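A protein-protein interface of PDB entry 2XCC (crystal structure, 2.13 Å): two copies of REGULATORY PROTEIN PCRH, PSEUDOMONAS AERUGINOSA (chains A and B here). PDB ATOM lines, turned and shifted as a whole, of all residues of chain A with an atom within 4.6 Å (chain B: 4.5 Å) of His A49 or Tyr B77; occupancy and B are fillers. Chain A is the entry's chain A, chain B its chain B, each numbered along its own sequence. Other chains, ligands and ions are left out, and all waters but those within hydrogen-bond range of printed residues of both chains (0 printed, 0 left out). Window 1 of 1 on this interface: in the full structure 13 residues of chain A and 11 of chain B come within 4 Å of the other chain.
Hydrophobic or aromatic side chains of chain B that line the printed part of chain A: Phe B55, Tyr B77, Leu B80 and Met B81.
Of the 10 printed residues of chain A, 6 touch a printed residue of chain B.
Hydrophobic or aromatic side chains of chain A within 4 Å of the printed part of chain B: Met A46, His A49, Phe A55, Tyr A77 and Met A81.
Of chain B, only Cys B45 (3.8 Å), Phe B55 (3.9 Å) and Tyr B77 (3.2 Å) come within 4 Å of His A49.
Of the printed residues of chain B, Met A81 touches Gln B73 (3.6 Å).
Of the printed residues of chain A, Gln B73 touches Tyr A77 (3.2 Å) and Met A81 (3.6 Å).
Printed residues of chain A within 4 Å of Met B81: Cys A45 (3.9 Å) and Met A46 (3.6 Å).
The nearest printed residue of chain B that does not touch Tyr A77 is Ser B76 (4.01 Å).
OH of Tyr B77 is in hydrogen-bond range of O of Cys A45 (2.7 Å).
SD of Met A46 lies close to OH of Tyr B77, 3.7 Å away.
SD of Met A81 sits close to OE1 of Gln B73, at 3.7 Å.
SD of Met A46 lies close to SD of Met B81 (3.6 Å).
OH of Tyr A77 sits at hydrogen-bond distance from O of His A49 (3.0 Å).
The side-chain hydroxyl (OH) of Tyr A77 sits close to the side-chain sulfur (SD) of Met A81, at 3.7 Å.
Cys A45 touches Met B81 (CB to CE, 3.9 Å).
Cys B45 touches His A49.
CZ of Phe B55 touches CE1 of His A49 (3.9 Å).
His A49 touches Tyr B77 (CD2 to OH, 3.2 Å).
CE1 of Phe A55 touches CD2 of Leu B80 (3.4 Å).
O of Gln B73 touches CE1 of Tyr A77, 3.2 Å away.
Tyr B77 touches Tyr A77 (CB to CE1, 3.6 Å).
Tyr A77 touches Leu B80 (CB to CD2, 3.97 Å).
Cys A45 touches Tyr B77, but with the chains exchanged Tyr A77 does not touch Cys B45 (9.5 Å).
Cys A45 touches Met B81, but with the chains exchanged Met A81 does not touch Cys B45 (10.2 Å).
Tyr B77 touches its own counterpart, Tyr A77.
Positions printed for both chains: 45, 55, 77 and 81.
Of the 12 pairs that touch across the chains among the printed residues, 1 has its exchanged pair printed and touching as well.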
ATOM      1  N   CYS A  45     -18.271  34.205  23.479  1.00  0.00           N
ATOM      2  CA  CYS A  45     -19.147  33.259  22.707  1.00  0.00           C
ATOM      3  C   CYS A  45     -18.403  32.517  21.625  1.00  0.00           C
ATOM      4  O   CYS A  45     -18.868  31.470  21.135  1.00  0.00           O
ATOM      5  CB  CYS A  45     -20.338  33.975  22.038  1.00  0.00           C
ATOM      6  SG  CYS A  45     -21.539  34.843  23.134  1.00  0.00           S
ATOM      7  N   MET A  46     -17.286  33.095  21.182  1.00  0.00           N
ATOM      8  CA  MET A  46     -16.305  32.401  20.312  1.00  0.00           C
ATOM      9  C   MET A  46     -15.558  31.299  21.092  1.00  0.00           C
ATOM     10  O   MET A  46     -15.354  30.210  20.588  1.00  0.00           O
ATOM     11  CB  MET A  46     -15.285  33.387  19.724  1.00  0.00           C
ATOM     12  CG  MET A  46     -15.734  34.215  18.474  1.00  0.00           C
ATOM     13  SD  MET A  46     -16.870  33.331  17.324  1.00  0.00           S
ATOM     14  CE  MET A  46     -15.967  31.876  16.764  1.00  0.00           C
ATOM     15  N   LEU A  47     -15.197  31.575  22.343  1.00  0.00           N
ATOM     16  CA  LEU A  47     -14.331  30.700  23.137  1.00  0.00           C
ATOM     17  C   LEU A  47     -15.067  29.566  23.885  1.00  0.00           C
ATOM     18  O   LEU A  47     -14.435  28.605  24.318  1.00  0.00           O
ATOM     19  CB  LEU A  47     -13.463  31.551  24.102  1.00  0.00           C
ATOM     20  CG  LEU A  47     -12.535  32.597  23.431  1.00  0.00           C
ATOM     21  CD1 LEU A  47     -11.930  33.636  24.376  1.00  0.00           C
ATOM     22  CD2 LEU A  47     -11.410  31.913  22.615  1.00  0.00           C
ATOM     23  N   ASP A  48     -16.386  29.673  24.027  1.00  0.00           N
ATOM     24  CA  ASP A  48     -17.215  28.613  24.617  1.00  0.00           C
ATOM     25  C   ASP A  48     -18.677  28.774  24.180  1.00  0.00           C
ATOM     26  O   ASP A  48     -19.433  29.639  24.706  1.00  0.00           O
ATOM     27  CB  ASP A  48     -17.124  28.636  26.143  1.00  0.00           C
ATOM     28  CG  ASP A  48     -17.819  27.448  26.790  1.00  0.00           C
ATOM     29  OD1 ASP A  48     -18.362  26.625  26.012  1.00  0.00           O
ATOM     30  OD2 ASP A  48     -17.788  27.323  28.062  1.00  0.00           O
ATOM     31  N   HIS A  49     -19.087  27.936  23.232  1.00  0.00           N
ATOM     32  CA  HIS A  49     -20.453  27.986  22.712  1.00  0.00           C
ATOM     33  C   HIS A  49     -21.486  27.280  23.586  1.00  0.00           C
ATOM     34  O   HIS A  49     -22.529  26.912  23.074  1.00  0.00           O
ATOM     35  CB  HIS A  49     -20.513  27.396  21.304  1.00  0.00           C
ATOM     36  CG  HIS A  49     -19.174  27.021  20.760  1.00  0.00           C
ATOM     37  ND1 HIS A  49     -18.762  25.710  20.648  1.00  0.00           N
ATOM     38  CD2 HIS A  49     -18.131  27.789  20.347  1.00  0.00           C
ATOM     39  CE1 HIS A  49     -17.534  25.686  20.152  1.00  0.00           C
ATOM     40  NE2 HIS A  49     -17.126  26.934  19.970  1.00  0.00           N
ATOM     41  N   TYR A  50     -21.213  27.080  24.881  1.00  0.00           N
ATOM     42  CA  TYR A  50     -22.220  26.527  25.796  1.00  0.00           C
ATOM     43  C   TYR A  50     -22.198  27.198  27.172  1.00  0.00           C
ATOM     44  O   TYR A  50     -22.226  26.536  28.207  1.00  0.00           O
ATOM     45  CB  TYR A  50     -22.080  25.005  25.967  1.00  0.00           C
ATOM     46  CG  TYR A  50     -21.114  24.297  25.045  1.00  0.00           C
ATOM     47  CD1 TYR A  50     -19.802  24.087  25.428  1.00  0.00           C
ATOM     48  CD2 TYR A  50     -21.523  23.803  23.827  1.00  0.00           C
ATOM     49  CE1 TYR A  50     -18.909  23.433  24.618  1.00  0.00           C
ATOM     50  CE2 TYR A  50     -20.642  23.147  23.003  1.00  0.00           C
ATOM     51  CZ  TYR A  50     -19.327  22.961  23.407  1.00  0.00           C
ATOM     52  OH  TYR A  50     -18.422  22.311  22.592  1.00  0.00           O
ATOM     53  N   ASP A  51     -22.130  28.511  27.206  1.00  0.00           N
ATOM     54  CA  ASP A  51     -22.323  29.178  28.485  1.00  0.00           C
ATOM     55  C   ASP A  51     -23.355  30.276  28.252  1.00  0.00           C
ATOM     56  O   ASP A  51     -23.000  31.434  27.997  1.00  0.00           O
ATOM     57  CB  ASP A  51     -21.009  29.691  29.073  1.00  0.00           C
ATOM     58  CG  ASP A  51     -21.085  29.917  30.576  1.00  0.00           C
ATOM     59  OD1 ASP A  51     -20.129  29.572  31.293  1.00  0.00           O
ATOM     60  OD2 ASP A  51     -22.096  30.432  31.077  1.00  0.00           O
ATOM     61  N   PHE A  55     -24.334  34.406  25.869  1.00  0.00           N
ATOM     62  CA  PHE A  55     -25.435  34.848  25.010  1.00  0.00           C
ATOM     63  C   PHE A  55     -26.406  35.754  25.743  1.00  0.00           C
ATOM     64  O   PHE A  55     -26.772  36.786  25.213  1.00  0.00           O
ATOM     65  CB  PHE A  55     -26.042  33.676  24.285  1.00  0.00           C
ATOM     66  CG  PHE A  55     -25.031  32.912  23.579  1.00  0.00           C
ATOM     67  CD1 PHE A  55     -24.744  33.176  22.260  1.00  0.00           C
ATOM     68  CD2 PHE A  55     -24.279  31.970  24.241  1.00  0.00           C
ATOM     69  CE1 PHE A  55     -23.726  32.449  21.605  1.00  0.00           C
ATOM     70  CE2 PHE A  55     -23.278  31.221  23.579  1.00  0.00           C
ATOM     71  CZ  PHE A  55     -23.024  31.474  22.273  1.00  0.00           C
ATOM     72  N   TYR A  77     -30.445  31.421  20.414  1.00  0.00           N
ATOM     73  CA  TYR A  77     -29.476  30.370  20.526  1.00  0.00           C
ATOM     74  C   TYR A  77     -29.300  30.041  22.017  1.00  0.00           C
ATOM     75  O   TYR A  77     -29.270  28.892  22.393  1.00  0.00           O
ATOM     76  CB  TYR A  77     -28.136  30.744  19.874  1.00  0.00           C
ATOM     77  CG  TYR A  77     -27.076  29.684  20.134  1.00  0.00           C
ATOM     78  CD1 TYR A  77     -27.094  28.487  19.425  1.00  0.00           C
ATOM     79  CD2 TYR A  77     -26.088  29.850  21.119  1.00  0.00           C
ATOM     80  CE1 TYR A  77     -26.152  27.506  19.631  1.00  0.00           C
ATOM     81  CE2 TYR A  77     -25.125  28.828  21.345  1.00  0.00           C
ATOM     82  CZ  TYR A  77     -25.186  27.673  20.567  1.00  0.00           C
ATOM     83  OH  TYR A  77     -24.324  26.629  20.740  1.00  0.00           O
ATOM     84  N   MET A  81     -29.754  26.394  24.294  1.00  0.00           N
ATOM     85  CA  MET A  81     -28.665  25.871  25.098  1.00  0.00           C
ATOM     86  C   MET A  81     -29.009  25.784  26.573  1.00  0.00           C
ATOM     87  O   MET A  81     -28.329  25.114  27.332  1.00  0.00           O
ATOM     88  CB  MET A  81     -27.372  26.703  24.889  1.00  0.00           C
ATOM     89  CG  MET A  81     -26.674  26.483  23.518  1.00  0.00           C
ATOM     90  SD  MET A  81     -26.954  24.882  22.706  1.00  0.00           S
ATOM     91  CE  MET A  81     -25.275  24.350  22.357  1.00  0.00           C
ATOM     92  N   CYS B  45     -14.422  21.205  16.724  1.00  0.00           N
ATOM     93  CA  CYS B  45     -15.053  22.513  17.045  1.00  0.00           C
ATOM     94  C   CYS B  45     -14.391  23.071  18.248  1.00  0.00           C
ATOM     95  O   CYS B  45     -14.405  24.289  18.483  1.00  0.00           O
ATOM     96  CB  CYS B  45     -16.558  22.412  17.352  1.00  0.00           C
ATOM     97  SG  CYS B  45     -17.520  21.988  15.913  1.00  0.00           S
ATOM     98  N   PHE B  55     -18.975  22.739  12.359  1.00  0.00           N
ATOM     99  CA  PHE B  55     -20.397  22.890  12.615  1.00  0.00           C
ATOM    100  C   PHE B  55     -21.295  22.359  11.505  1.00  0.00           C
ATOM    101  O   PHE B  55     -22.270  21.656  11.783  1.00  0.00           O
ATOM    102  CB  PHE B  55     -20.658  24.347  12.856  1.00  0.00           C
ATOM    103  CG  PHE B  55     -19.929  24.853  14.075  1.00  0.00           C
ATOM    104  CD1 PHE B  55     -20.399  24.534  15.331  1.00  0.00           C
ATOM    105  CD2 PHE B  55     -18.727  25.588  13.953  1.00  0.00           C
ATOM    106  CE1 PHE B  55     -19.730  25.009  16.489  1.00  0.00           C
ATOM    107  CE2 PHE B  55     -18.046  26.043  15.108  1.00  0.00           C
ATOM    108  CZ  PHE B  55     -18.565  25.766  16.357  1.00  0.00           C
ATOM    109  N   GLN B  73     -29.128  23.411  17.211  1.00  0.00           N
ATOM    110  CA  GLN B  73     -28.080  24.098  17.999  1.00  0.00           C
ATOM    111  C   GLN B  73     -26.827  24.342  17.185  1.00  0.00           C
ATOM    112  O   GLN B  73     -26.342  25.468  17.111  1.00  0.00           O
ATOM    113  CB  GLN B  73     -27.655  23.246  19.217  1.00  0.00           C
ATOM    114  CG  GLN B  73     -28.839  22.854  20.127  1.00  0.00           C
ATOM    115  CD  GLN B  73     -28.472  21.901  21.293  1.00  0.00           C
ATOM    116  OE1 GLN B  73     -27.352  21.416  21.410  1.00  0.00           O
ATOM    117  NE2 GLN B  73     -29.438  21.632  22.135  1.00  0.00           N
ATOM    118  N   SER B  74     -26.326  23.285  16.549  1.00  0.00           N
ATOM    119  CA  SER B  74     -25.141  23.425  15.735  1.00  0.00           C
ATOM    120  C   SER B  74     -25.334  24.496  14.682  1.00  0.00           C
ATOM    121  O   SER B  74     -24.547  25.449  14.624  1.00  0.00           O
ATOM    122  CB  SER B  74     -24.707  22.097  15.093  1.00  0.00           C
ATOM    123  OG  SER B  74     -24.335  21.130  16.073  1.00  0.00           O
ATOM    124  N   TYR B  75     -26.375  24.372  13.865  1.00  0.00           N
ATOM    125  CA  TYR B  75     -26.534  25.263  12.679  1.00  0.00           C
ATOM    126  C   TYR B  75     -26.850  26.656  13.145  1.00  0.00           C
ATOM    127  O   TYR B  75     -26.499  27.631  12.506  1.00  0.00           O
ATOM    128  CB  TYR B  75     -27.663  24.792  11.760  1.00  0.00           C
ATOM    129  CG  TYR B  75     -27.482  23.450  11.107  1.00  0.00           C
ATOM    130  CD1 TYR B  75     -26.373  23.188  10.302  1.00  0.00           C
ATOM    131  CD2 TYR B  75     -28.449  22.450  11.251  1.00  0.00           C
ATOM    132  CE1 TYR B  75     -26.202  21.908   9.680  1.00  0.00           C
ATOM    133  CE2 TYR B  75     -28.283  21.136  10.634  1.00  0.00           C
ATOM    134  CZ  TYR B  75     -27.144  20.909   9.839  1.00  0.00           C
ATOM    135  OH  TYR B  75     -26.944  19.713   9.171  1.00  0.00           O
ATOM    136  N   SER B  76     -27.501  26.742  14.302  1.00  0.00           N
ATOM    137  CA  SER B  76     -27.872  28.043  14.863  1.00  0.00           C
ATOM    138  C   SER B  76     -26.678  28.763  15.449  1.00  0.00           C
ATOM    139  O   SER B  76     -26.641  29.990  15.471  1.00  0.00           O
ATOM    140  CB  SER B  76     -28.974  27.907  15.912  1.00  0.00           C
ATOM    141  OG  SER B  76     -30.057  27.173  15.411  1.00  0.00           O
ATOM    142  N   TYR B  77     -25.692  28.018  15.936  1.00  0.00           N
ATOM    143  CA  TYR B  77     -24.424  28.638  16.321  1.00  0.00           C
ATOM    144  C   TYR B  77     -23.720  29.059  15.037  1.00  0.00           C
ATOM    145  O   TYR B  77     -23.305  30.189  14.909  1.00  0.00           O
ATOM    146  CB  TYR B  77     -23.534  27.692  17.132  1.00  0.00           C
ATOM    147  CG  TYR B  77     -22.278  28.383  17.571  1.00  0.00           C
ATOM    148  CD1 TYR B  77     -22.306  29.294  18.606  1.00  0.00           C
ATOM    149  CD2 TYR B  77     -21.095  28.207  16.883  1.00  0.00           C
ATOM    150  CE1 TYR B  77     -21.164  29.977  18.979  1.00  0.00           C
ATOM    151  CE2 TYR B  77     -19.933  28.860  17.265  1.00  0.00           C
ATOM    152  CZ  TYR B  77     -19.973  29.757  18.291  1.00  0.00           C
ATOM    153  OH  TYR B  77     -18.825  30.434  18.635  1.00  0.00           O
ATOM    154  N   GLY B  78     -23.627  28.170  14.067  1.00  0.00           N
ATOM    155  CA  GLY B  78     -23.081  28.571  12.769  1.00  0.00           C
ATOM    156  C   GLY B  78     -23.630  29.907  12.284  1.00  0.00           C
ATOM    157  O   GLY B  78     -22.872  30.841  12.040  1.00  0.00           O
ATOM    158  N   ALA B  79     -24.942  30.030  12.143  1.00  0.00           N
ATOM    159  CA  ALA B  79     -25.563  31.295  11.615  1.00  0.00           C
ATOM    160  C   ALA B  79     -25.363  32.504  12.537  1.00  0.00           C
ATOM    161  O   ALA B  79     -25.440  33.684  12.116  1.00  0.00           O
ATOM    162  CB  ALA B  79     -27.023  31.111  11.392  1.00  0.00           C
ATOM    163  N   LEU B  80     -25.126  32.231  13.806  1.00  0.00           N
ATOM    164  CA  LEU B  80     -24.972  33.326  14.749  1.00  0.00           C
ATOM    165  C   LEU B  80     -23.610  33.976  14.591  1.00  0.00           C
ATOM    166  O   LEU B  80     -23.419  35.124  14.923  1.00  0.00           O
ATOM    167  CB  LEU B  80     -25.113  32.783  16.163  1.00  0.00           C
ATOM    168  CG  LEU B  80     -25.124  33.799  17.284  1.00  0.00           C
ATOM    169  CD1 LEU B  80     -26.298  34.765  17.197  1.00  0.00           C
ATOM    170  CD2 LEU B  80     -25.168  33.027  18.555  1.00  0.00           C
ATOM    171  N   MET B  81     -22.656  33.228  14.060  1.00  0.00           N
ATOM    172  CA  MET B  81     -21.281  33.687  14.018  1.00  0.00           C
ATOM    173  C   MET B  81     -20.915  33.964  12.604  1.00  0.00           C
ATOM    174  O   MET B  81     -19.962  34.686  12.343  1.00  0.00           O
ATOM    175  CB  MET B  81     -20.361  32.608  14.606  1.00  0.00           C
ATOM    176  CG  MET B  81     -20.747  32.266  16.038  1.00  0.00           C
ATOM    177  SD  MET B  81     -20.441  33.735  17.052  1.00  0.00           S
ATOM    178  CE  MET B  81     -21.656  33.636  18.345  1.00  0.00           C
